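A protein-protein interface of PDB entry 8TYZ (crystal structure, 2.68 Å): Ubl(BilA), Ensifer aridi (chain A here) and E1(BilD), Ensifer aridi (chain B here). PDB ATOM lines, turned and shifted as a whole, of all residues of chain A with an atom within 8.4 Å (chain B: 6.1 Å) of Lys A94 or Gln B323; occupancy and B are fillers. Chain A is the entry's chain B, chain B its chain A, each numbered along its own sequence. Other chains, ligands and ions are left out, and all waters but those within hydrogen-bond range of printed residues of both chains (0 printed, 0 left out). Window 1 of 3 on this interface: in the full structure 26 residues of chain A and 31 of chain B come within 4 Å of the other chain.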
ATOM      1  N   ASN A  27      21.284 -30.023 -26.345  1.00  0.00           N
ATOM      2  CA  ASN A  27      20.045 -29.744 -27.079  1.00  0.00           C
ATOM      3  C   ASN A  27      19.324 -31.062 -27.362  1.00  0.00           C
ATOM      4  O   ASN A  27      18.828 -31.305 -28.460  1.00  0.00           O
ATOM      5  CB  ASN A  27      20.334 -28.964 -28.366  1.00  0.00           C
ATOM      6  CG  ASN A  27      19.108 -28.308 -28.961  1.00  0.00           C
ATOM      7  OD1 ASN A  27      18.165 -27.938 -28.258  1.00  0.00           O
ATOM      8  ND2 ASN A  27      19.131 -28.126 -30.280  1.00  0.00           N
ATOM      9  N   GLN A  57      25.716 -21.285 -33.750  1.00  0.00           N
ATOM     10  CA  GLN A  57      25.428 -20.335 -32.672  1.00  0.00           C
ATOM     11  C   GLN A  57      26.711 -19.968 -31.912  1.00  0.00           C
ATOM     12  O   GLN A  57      27.606 -20.809 -31.748  1.00  0.00           O
ATOM     13  CB  GLN A  57      24.404 -20.929 -31.687  1.00  0.00           C
ATOM     14  CG  GLN A  57      23.027 -21.221 -32.239  1.00  0.00           C
ATOM     15  CD  GLN A  57      22.035 -20.071 -31.989  1.00  0.00           C
ATOM     16  OE1 GLN A  57      22.321 -19.143 -31.222  1.00  0.00           O
ATOM     17  NE2 GLN A  57      20.866 -20.129 -32.642  1.00  0.00           N
ATOM     18  N   ASP A  60      28.418 -18.830 -26.205  1.00  0.00           N
ATOM     19  CA  ASP A  60      27.825 -18.182 -25.033  1.00  0.00           C
ATOM     20  C   ASP A  60      26.309 -18.327 -24.991  1.00  0.00           C
ATOM     21  O   ASP A  60      25.705 -18.101 -23.938  1.00  0.00           O
ATOM     22  CB  ASP A  60      28.185 -16.697 -25.007  1.00  0.00           C
ATOM     23  CG  ASP A  60      29.637 -16.443 -24.580  1.00  0.00           C
ATOM     24  OD1 ASP A  60      30.404 -17.426 -24.397  1.00  0.00           O
ATOM     25  OD2 ASP A  60      30.006 -15.251 -24.418  1.00  0.00           O
ATOM     26  N   ASN A  61      25.684 -18.671 -26.118  1.00  0.00           N
ATOM     27  CA  ASN A  61      24.259 -18.945 -26.147  1.00  0.00           C
ATOM     28  C   ASN A  61      23.889 -20.204 -25.384  1.00  0.00           C
ATOM     29  O   ASN A  61      22.707 -20.400 -25.087  1.00  0.00           O
ATOM     30  CB  ASN A  61      23.797 -19.069 -27.591  1.00  0.00           C
ATOM     31  CG  ASN A  61      23.939 -17.772 -28.347  1.00  0.00           C
ATOM     32  OD1 ASN A  61      24.691 -16.894 -27.932  1.00  0.00           O
ATOM     33  ND2 ASN A  61      23.204 -17.631 -29.456  1.00  0.00           N
ATOM     34  N   TRP A  62      24.857 -21.064 -25.081  1.00  0.00           N
ATOM     35  CA  TRP A  62      24.589 -22.335 -24.438  1.00  0.00           C
ATOM     36  C   TRP A  62      24.760 -22.185 -22.939  1.00  0.00           C
ATOM     37  O   TRP A  62      25.682 -21.513 -22.474  1.00  0.00           O
ATOM     38  CB  TRP A  62      25.513 -23.422 -24.991  1.00  0.00           C
ATOM     39  CG  TRP A  62      25.273 -23.697 -26.452  1.00  0.00           C
ATOM     40  CD1 TRP A  62      25.966 -23.181 -27.508  1.00  0.00           C
ATOM     41  CD2 TRP A  62      24.256 -24.537 -27.010  1.00  0.00           C
ATOM     42  NE1 TRP A  62      25.440 -23.645 -28.688  1.00  0.00           N
ATOM     43  CE2 TRP A  62      24.390 -24.478 -28.414  1.00  0.00           C
ATOM     44  CE3 TRP A  62      23.250 -25.343 -26.459  1.00  0.00           C
ATOM     45  CZ2 TRP A  62      23.552 -25.192 -29.283  1.00  0.00           C
ATOM     46  CZ3 TRP A  62      22.417 -26.053 -27.321  1.00  0.00           C
ATOM     47  CH2 TRP A  62      22.576 -25.972 -28.719  1.00  0.00           C
ATOM     48  N   GLU A  63      23.830 -22.768 -22.188  1.00  0.00           N
ATOM     49  CA  GLU A  63      23.898 -22.806 -20.735  1.00  0.00           C
ATOM     50  C   GLU A  63      24.390 -24.177 -20.303  1.00  0.00           C
ATOM     51  O   GLU A  63      23.698 -25.179 -20.523  1.00  0.00           O
ATOM     52  CB  GLU A  63      22.540 -22.529 -20.094  1.00  0.00           C
ATOM     53  CG  GLU A  63      21.972 -21.154 -20.387  1.00  0.00           C
ATOM     54  CD  GLU A  63      20.808 -20.803 -19.481  1.00  0.00           C
ATOM     55  OE1 GLU A  63      19.967 -21.696 -19.191  1.00  0.00           O
ATOM     56  OE2 GLU A  63      20.743 -19.630 -19.046  1.00  0.00           O
ATOM     57  N   LYS A  65      24.712 -26.640 -17.509  1.00  0.00           N
ATOM     58  CA  LYS A  65      23.981 -26.868 -16.273  1.00  0.00           C
ATOM     59  C   LYS A  65      24.198 -28.296 -15.806  1.00  0.00           C
ATOM     60  O   LYS A  65      24.394 -29.205 -16.617  1.00  0.00           O
ATOM     61  CB  LYS A  65      22.452 -26.647 -16.437  1.00  0.00           C
ATOM     62  CG  LYS A  65      22.056 -25.431 -17.243  1.00  0.00           C
ATOM     63  CD  LYS A  65      20.563 -25.383 -17.485  1.00  0.00           C
ATOM     64  CE  LYS A  65      20.100 -26.422 -18.509  1.00  0.00           C
ATOM     65  NZ  LYS A  65      18.816 -26.031 -19.165  1.00  0.00           N
ATOM     66  N   LEU A  71      23.340 -23.371 -13.090  1.00  0.00           N
ATOM     67  CA  LEU A  71      24.219 -22.865 -14.139  1.00  0.00           C
ATOM     68  C   LEU A  71      25.687 -22.883 -13.685  1.00  0.00           C
ATOM     69  O   LEU A  71      26.041 -22.309 -12.647  1.00  0.00           O
ATOM     70  CB  LEU A  71      23.781 -21.464 -14.569  1.00  0.00           C
ATOM     71  CG  LEU A  71      24.180 -21.022 -15.987  1.00  0.00           C
ATOM     72  CD1 LEU A  71      23.196 -20.069 -16.613  1.00  0.00           C
ATOM     73  CD2 LEU A  71      25.567 -20.371 -15.999  1.00  0.00           C
ATOM     74  N   LEU A  91      23.766 -29.111 -21.870  1.00  0.00           N
ATOM     75  CA  LEU A  91      24.134 -27.939 -22.666  1.00  0.00           C
ATOM     76  C   LEU A  91      22.872 -27.496 -23.400  1.00  0.00           C
ATOM     77  O   LEU A  91      22.532 -28.032 -24.458  1.00  0.00           O
ATOM     78  CB  LEU A  91      25.270 -28.257 -23.630  1.00  0.00           C
ATOM     79  CG  LEU A  91      26.357 -27.224 -23.886  1.00  0.00           C
ATOM     80  CD1 LEU A  91      26.815 -26.718 -22.571  1.00  0.00           C
ATOM     81  CD2 LEU A  91      27.509 -27.892 -24.612  1.00  0.00           C
ATOM     82  N   SER A  92      22.165 -26.526 -22.836  1.00  0.00           N
ATOM     83  CA  SER A  92      20.818 -26.212 -23.274  1.00  0.00           C
ATOM     84  C   SER A  92      20.706 -24.744 -23.650  1.00  0.00           C
ATOM     85  O   SER A  92      21.399 -23.885 -23.097  1.00  0.00           O
ATOM     86  CB  SER A  92      19.810 -26.554 -22.184  1.00  0.00           C
ATOM     87  OG  SER A  92      19.896 -27.932 -21.875  1.00  0.00           O
ATOM     88  N   LEU A  93      19.844 -24.462 -24.614  1.00  0.00           N
ATOM     89  CA  LEU A  93      19.633 -23.073 -24.971  1.00  0.00           C
ATOM     90  C   LEU A  93      18.815 -22.379 -23.877  1.00  0.00           C
ATOM     91  O   LEU A  93      18.172 -23.025 -23.041  1.00  0.00           O
ATOM     92  CB  LEU A  93      18.960 -22.968 -26.347  1.00  0.00           C
ATOM     93  CG  LEU A  93      19.866 -23.274 -27.551  1.00  0.00           C
ATOM     94  CD1 LEU A  93      19.103 -23.415 -28.846  1.00  0.00           C
ATOM     95  CD2 LEU A  93      20.905 -22.194 -27.698  1.00  0.00           C
ATOM     96  N   LYS A  94      18.898 -21.048 -23.846  1.00  0.00           N
ATOM     97  CA  LYS A  94      17.966 -20.279 -23.034  1.00  0.00           C
ATOM     98  C   LYS A  94      16.542 -20.544 -23.513  1.00  0.00           C
ATOM     99  O   LYS A  94      16.305 -20.809 -24.693  1.00  0.00           O
ATOM    100  CB  LYS A  94      18.292 -18.784 -23.115  1.00  0.00           C
ATOM    101  CG  LYS A  94      19.482 -18.384 -22.300  1.00  0.00           C
ATOM    102  CD  LYS A  94      19.715 -16.892 -22.282  1.00  0.00           C
ATOM    103  CE  LYS A  94      20.703 -16.557 -21.167  1.00  0.00           C
ATOM    104  NZ  LYS A  94      20.715 -15.134 -20.724  1.00  0.00           N
ATOM    105  N   ALA A  95      15.586 -20.501 -22.586  1.00  0.00           N
ATOM    106  CA  ALA A  95      14.194 -20.686 -22.973  1.00  0.00           C
ATOM    107  C   ALA A  95      13.785 -19.606 -23.969  1.00  0.00           C
ATOM    108  O   ALA A  95      14.232 -18.465 -23.891  1.00  0.00           O
ATOM    109  CB  ALA A  95      13.299 -20.670 -21.746  1.00  0.00           C
ATOM    110  N   GLY A  96      12.985 -19.988 -24.949  1.00  0.00           N
ATOM    111  CA  GLY A  96      12.671 -19.083 -26.030  1.00  0.00           C
ATOM    112  C   GLY A  96      11.574 -18.137 -25.638  1.00  0.00           C
ATOM    113  O   GLY A  96      10.951 -18.288 -24.594  1.00  0.00           O
ATOM    114  N   VAL A  97      11.337 -17.144 -26.489  1.00  0.00           N
ATOM    115  CA  VAL A  97      10.239 -16.213 -26.258  1.00  0.00           C
ATOM    116  C   VAL A  97       9.173 -16.249 -27.350  1.00  0.00           C
ATOM    117  O   VAL A  97       8.072 -15.732 -27.114  1.00  0.00           O
ATOM    118  CB  VAL A  97      10.756 -14.774 -26.052  1.00  0.00           C
ATOM    119  CG1 VAL A  97      11.733 -14.713 -24.901  1.00  0.00           C
ATOM    120  CG2 VAL A  97      11.365 -14.213 -27.329  1.00  0.00           C
ATOM    121  N   ALA A  98       9.419 -16.871 -28.508  1.00  0.00           N
ATOM    122  CA  ALA A  98       8.492 -16.785 -29.637  1.00  0.00           C
ATOM    123  C   ALA A  98       7.304 -17.723 -29.450  1.00  0.00           C
ATOM    124  O   ALA A  98       7.476 -18.874 -29.053  1.00  0.00           O
ATOM    125  CB  ALA A  98       9.199 -17.116 -30.960  1.00  0.00           C
ATOM    126  N   GLY A  99       6.098 -17.232 -29.755  1.00  0.00           N
ATOM    127  CA  GLY A  99       4.880 -18.017 -29.652  1.00  0.00           C
ATOM    128  C   GLY A  99       3.769 -17.636 -30.615  1.00  0.00           C
ATOM    129  O   GLY A  99       2.907 -18.462 -30.949  1.00  0.00           O
ATOM    130  N   TRP B 321       7.146 -22.299 -26.129  1.00  0.00           N
ATOM    131  CA  TRP B 321       7.967 -21.432 -26.963  1.00  0.00           C
ATOM    132  C   TRP B 321       8.511 -22.202 -28.166  1.00  0.00           C
ATOM    133  O   TRP B 321       8.556 -23.430 -28.168  1.00  0.00           O
ATOM    134  CB  TRP B 321       9.118 -20.810 -26.153  1.00  0.00           C
ATOM    135  CG  TRP B 321      10.162 -21.791 -25.758  1.00  0.00           C
ATOM    136  CD1 TRP B 321      11.182 -22.260 -26.537  1.00  0.00           C
ATOM    137  CD2 TRP B 321      10.286 -22.456 -24.495  1.00  0.00           C
ATOM    138  NE1 TRP B 321      11.926 -23.187 -25.840  1.00  0.00           N
ATOM    139  CE2 TRP B 321      11.399 -23.324 -24.583  1.00  0.00           C
ATOM    140  CE3 TRP B 321       9.558 -22.420 -23.312  1.00  0.00           C
ATOM    141  CZ2 TRP B 321      11.810 -24.123 -23.515  1.00  0.00           C
ATOM    142  CZ3 TRP B 321       9.964 -23.216 -22.258  1.00  0.00           C
ATOM    143  CH2 TRP B 321      11.081 -24.048 -22.362  1.00  0.00           C
ATOM    144  N   THR B 322       8.926 -21.456 -29.194  1.00  0.00           N
ATOM    145  CA  THR B 322       9.745 -21.961 -30.296  1.00  0.00           C
ATOM    146  C   THR B 322      10.858 -20.968 -30.635  1.00  0.00           C
ATOM    147  O   THR B 322      10.608 -19.764 -30.734  1.00  0.00           O
ATOM    148  CB  THR B 322       8.906 -22.211 -31.562  1.00  0.00           C
ATOM    149  OG1 THR B 322       8.285 -20.995 -31.970  1.00  0.00           O
ATOM    150  CG2 THR B 322       7.845 -23.224 -31.304  1.00  0.00           C
ATOM    151  N   GLN B 323      12.086 -21.465 -30.820  1.00  0.00           N
ATOM    152  CA  GLN B 323      13.229 -20.682 -31.314  1.00  0.00           C
ATOM    153  C   GLN B 323      13.868 -21.408 -32.498  1.00  0.00           C
ATOM    154  O   GLN B 323      13.244 -22.280 -33.111  1.00  0.00           O
ATOM    155  CB  GLN B 323      14.227 -20.416 -30.200  1.00  0.00           C
ATOM    156  CG  GLN B 323      14.706 -21.587 -29.396  1.00  0.00           C
ATOM    157  CD  GLN B 323      15.318 -21.113 -28.110  1.00  0.00           C
ATOM    158  OE1 GLN B 323      15.712 -19.955 -28.011  1.00  0.00           O
ATOM    159  NE2 GLN B 323      15.371 -21.979 -27.100  1.00  0.00           N
ATOM    160  N   GLU B 324      15.100 -21.044 -32.830  1.00  0.00           N
ATOM    161  CA  GLU B 324      15.660 -21.525 -34.087  1.00  0.00           C
ATOM    162  C   GLU B 324      15.924 -23.031 -34.044  1.00  0.00           C
ATOM    163  O   GLU B 324      15.484 -23.782 -34.932  1.00  0.00           O
ATOM    164  CB  GLU B 324      16.923 -20.718 -34.423  1.00  0.00           C
ATOM    165  CG  GLU B 324      16.721 -19.180 -34.240  1.00  0.00           C
ATOM    166  CD  GLU B 324      17.489 -18.295 -35.247  1.00  0.00           C
ATOM    167  OE1 GLU B 324      18.553 -18.733 -35.755  1.00  0.00           O
ATOM    168  OE2 GLU B 324      17.018 -17.154 -35.531  1.00  0.00           O
ATOM    169  N   HIS B 325      16.613 -23.495 -33.008  1.00  0.00           N
ATOM    170  CA  HIS B 325      17.051 -24.881 -32.942  1.00  0.00           C
ATOM    171  C   HIS B 325      16.291 -25.683 -31.904  1.00  0.00           C
ATOM    172  O   HIS B 325      16.777 -26.735 -31.466  1.00  0.00           O
ATOM    173  CB  HIS B 325      18.549 -24.915 -32.659  1.00  0.00           C
ATOM    174  CG  HIS B 325      19.339 -24.282 -33.745  1.00  0.00           C
ATOM    175  ND1 HIS B 325      19.840 -23.001 -33.650  1.00  0.00           N
ATOM    176  CD2 HIS B 325      19.620 -24.708 -34.999  1.00  0.00           C
ATOM    177  CE1 HIS B 325      20.440 -22.684 -34.781  1.00  0.00           C
ATOM    178  NE2 HIS B 325      20.317 -23.702 -35.618  1.00  0.00           N
ATOM    179  N   ASP B 326      15.105 -25.219 -31.509  1.00  0.00           N
ATOM    180  CA  ASP B 326      14.504 -25.762 -30.303  1.00  0.00           C
ATOM    181  C   ASP B 326      13.073 -25.249 -30.139  1.00  0.00           C
ATOM    182  O   ASP B 326      12.712 -24.183 -30.651  1.00  0.00           O
ATOM    183  CB  ASP B 326      15.394 -25.399 -29.109  1.00  0.00           C
ATOM    184  CG  ASP B 326      14.671 -25.434 -27.806  1.00  0.00           C
ATOM    185  OD1 ASP B 326      14.565 -26.552 -27.219  1.00  0.00           O
ATOM    186  OD2 ASP B 326      14.271 -24.328 -27.339  1.00  0.00           O
ATOM    187  N   LEU B 327      12.260 -26.064 -29.462  1.00  0.00           N
ATOM    188  CA  LEU B 327      10.919 -25.742 -28.979  1.00  0.00           C
ATOM    189  C   LEU B 327      10.750 -26.474 -27.659  1.00  0.00           C
ATOM    190  O   LEU B 327      11.348 -27.528 -27.448  1.00  0.00           O
ATOM    191  CB  LEU B 327       9.802 -26.180 -29.963  1.00  0.00           C
ATOM    192  CG  LEU B 327       9.546 -27.684 -30.209  1.00  0.00           C
ATOM    193  CD1 LEU B 327       8.677 -28.327 -29.172  1.00  0.00           C
ATOM    194  CD2 LEU B 327       8.976 -27.928 -31.574  1.00  0.00           C
ATOM    195  N   MET B 344      12.865 -18.444 -15.731  1.00  0.00           N
ATOM    196  CA  MET B 344      13.213 -18.793 -17.093  1.00  0.00           C
ATOM    197  C   MET B 344      13.725 -17.603 -17.884  1.00  0.00           C
ATOM    198  O   MET B 344      14.484 -17.788 -18.844  1.00  0.00           O
ATOM    199  CB  MET B 344      11.979 -19.400 -17.753  1.00  0.00           C
ATOM    200  CG  MET B 344      11.363 -20.479 -16.888  1.00  0.00           C
ATOM    201  SD  MET B 344      12.433 -21.907 -16.671  1.00  0.00           S
ATOM    202  CE  MET B 344      12.803 -22.203 -18.385  1.00  0.00           C
ATOM    203  N   MET B 346      14.929 -14.550 -16.325  1.00  0.00           N
ATOM    204  CA  MET B 346      15.763 -13.649 -15.535  1.00  0.00           C
ATOM    205  C   MET B 346      16.951 -13.151 -16.357  1.00  0.00           C
ATOM    206  O   MET B 346      17.494 -13.894 -17.185  1.00  0.00           O
ATOM    207  CB  MET B 346      16.272 -14.350 -14.278  1.00  0.00           C
ATOM    208  CG  MET B 346      15.260 -14.362 -13.164  1.00  0.00           C
ATOM    209  SD  MET B 346      14.795 -12.730 -12.548  1.00  0.00           S
ATOM    210  CE  MET B 346      16.166 -12.323 -11.478  1.00  0.00           C
ATOM    211  N   PRO B 347      17.365 -11.905 -16.182  1.00  0.00           N
ATOM    212  CA  PRO B 347      18.530 -11.414 -16.913  1.00  0.00           C
ATOM    213  C   PRO B 347      19.818 -11.913 -16.281  1.00  0.00           C
ATOM    214  O   PRO B 347      19.904 -12.142 -15.069  1.00  0.00           O
ATOM    215  CB  PRO B 347      18.404  -9.894 -16.796  1.00  0.00           C
ATOM    216  CG  PRO B 347      17.752  -9.712 -15.524  1.00  0.00           C
ATOM    217  CD  PRO B 347      16.785 -10.855 -15.338  1.00  0.00           C
ATOM    218  N   SER B 348      20.808 -12.109 -17.145  1.00  0.00           N
ATOM    219  CA  SER B 348      22.113 -12.631 -16.782  1.00  0.00           C
ATOM    220  C   SER B 348      23.088 -11.480 -16.589  1.00  0.00           C
ATOM    221  O   SER B 348      22.937 -10.402 -17.173  1.00  0.00           O
ATOM    222  CB  SER B 348      22.641 -13.603 -17.852  1.00  0.00           C
ATOM    223  OG  SER B 348      22.427 -13.118 -19.173  1.00  0.00           O
ATOM    224  N   VAL B 434      12.283 -13.925 -35.217  1.00  0.00           N
ATOM    225  CA  VAL B 434      12.373 -15.364 -35.438  1.00  0.00           C
ATOM    226  C   VAL B 434      11.014 -15.881 -35.900  1.00  0.00           C
ATOM    227  O   VAL B 434      10.045 -15.880 -35.139  1.00  0.00           O
ATOM    228  CB  VAL B 434      12.857 -16.096 -34.185  1.00  0.00           C
ATOM    229  CG1 VAL B 434      12.584 -17.577 -34.323  1.00  0.00           C
ATOM    230  CG2 VAL B 434      14.348 -15.840 -34.011  1.00  0.00           C
ATOM    231  N   PRO B 436       9.117 -19.174 -36.913  1.00  0.00           N
ATOM    232  CA  PRO B 436       9.299 -20.617 -36.806  1.00  0.00           C
ATOM    233  C   PRO B 436       8.582 -21.395 -37.902  1.00  0.00           C
ATOM    234  O   PRO B 436       7.667 -20.895 -38.573  1.00  0.00           O
ATOM    235  CB  PRO B 436       8.686 -20.927 -35.436  1.00  0.00           C
ATOM    236  CG  PRO B 436       7.586 -19.987 -35.365  1.00  0.00           C
ATOM    237  CD  PRO B 436       8.084 -18.696 -35.974  1.00  0.00           C
ATOM    238  N   GLN B 440       6.978 -26.739 -35.970  1.00  0.00           N
ATOM    239  CA  GLN B 440       7.400 -26.449 -34.598  1.00  0.00           C
ATOM    240  C   GLN B 440       6.233 -25.874 -33.798  1.00  0.00           C
ATOM    241  O   GLN B 440       5.895 -26.358 -32.713  1.00  0.00           O
ATOM    242  CB  GLN B 440       8.571 -25.470 -34.571  1.00  0.00           C
ATOM    243  CG  GLN B 440       9.856 -25.843 -35.283  1.00  0.00           C
ATOM    244  CD  GLN B 440      10.819 -24.667 -35.238  1.00  0.00           C
ATOM    245  OE1 GLN B 440      10.835 -23.812 -36.124  1.00  0.00           O
ATOM    246  NE2 GLN B 440      11.573 -24.586 -34.162  1.00  0.00           N
ATOM    247  N   ARG B 468      12.027 -30.282 -24.048  1.00  0.00           N
ATOM    248  CA  ARG B 468      12.377 -29.583 -25.274  1.00  0.00           C
ATOM    249  C   ARG B 468      12.527 -30.560 -26.432  1.00  0.00           C
ATOM    250  O   ARG B 468      12.788 -31.752 -26.224  1.00  0.00           O
ATOM    251  CB  ARG B 468      13.645 -28.809 -25.099  1.00  0.00           C
ATOM    252  CG  ARG B 468      13.662 -27.784 -23.998  1.00  0.00           C
ATOM    253  CD  ARG B 468      15.057 -27.300 -24.014  1.00  0.00           C
ATOM    254  NE  ARG B 468      15.384 -26.098 -23.278  1.00  0.00           N
ATOM    255  CZ  ARG B 468      15.586 -24.923 -23.844  1.00  0.00           C
ATOM    256  NH1 ARG B 468      15.296 -24.711 -25.109  1.00  0.00           N
ATOM    257  NH2 ARG B 468      16.093 -23.935 -23.118  1.00  0.00           N
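The backbone NH (N) of Thr B322 lies within hydrogen-bond range of the backbone carbonyl oxygen (O) of Ala A98 (3.0 Å).
The guanidinium group of Arg B468 lies close to the backbone carbonyl oxygen of Leu A93 (2.3 Å).
N of Gly A96 sits close to NE1 of Trp B321, at 3.5 Å.
The side-chain hydroxyl (OG) of Ser B348 lies within hydrogen-bond range of the side-chain amino group (NZ) of Lys A94.
NE2 of Gln B323 lies within hydrogen-bond range of O of Lys A94 (2.8 Å).
ND1 of His B325 is in hydrogen-bond range of NE2 of Gln A57 (3.2 Å).
The side-chain amide nitrogen (ND2) of Asn A27 sits at hydrogen-bond distance from the backbone carbonyl oxygen (O) of His B325, 3.0 Å away.
OD2 of Asp B326 is in salt-bridge range of NH1 of Arg B468.
The side-chain amide nitrogen (ND2) of Asn A61 lies within hydrogen-bond range of the side-chain amide oxygen (OE1) of Gln A57.
The side-chain amide nitrogen (NE2) of Gln B440 sits at hydrogen-bond distance from the backbone carbonyl oxygen (O) of Gln B323, at 3.0 Å.
The indole nitrogen of Trp B321 is in hydrogen-bond range of the side-chain carboxylate of Asp B326 (3.0 Å).
The backbone carbonyl oxygen (O) of Leu A91 is in hydrogen-bond range of the backbone NH (N) of Asn A27.
The guanidinium group of Arg B468 sits close to the side-chain amide nitrogen of Gln B323 (3.4 Å).
Among the printed residues, pairs that only touch across the chains: Asn A27 with Asp B326 (3.9 Å), Leu A93 with Gln B323 (3.8 Å), Lys A94 with Arg B468 (3.4 Å), Ala A95 with Met B344 (3.7 Å), Ala A95 with Arg B468 (3.5 Å), Gly A96 with Gln B323 (3.7 Å) and Ala A98 with Trp B321 (3.3 Å).
Of the printed residues of chain B, Asn A27 touches His B325 (3.0 Å) and Asp B326 (3.9 Å).
Of the printed residues of chain B, Ala A95 touches Met B344 and Arg B468.
Printed residues of chain B within 4 Å of Gly A96: Trp B321 and Gln B323.
Gln B323 touches three residues of chain A.
The nearest residue of chain A that does not touch Gln B323 is Ala A95 (4.2 Å).
Of the 17 printed residues of chain A, 7 touch a printed residue of chain B.
Hydrophobic or aromatic side chains of chain A that line the printed part of chain B: Leu A93, Ala A95 and Ala A98.
Along chain A the printed residues that touch a printed residue of chain B span positions 27 to 98.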
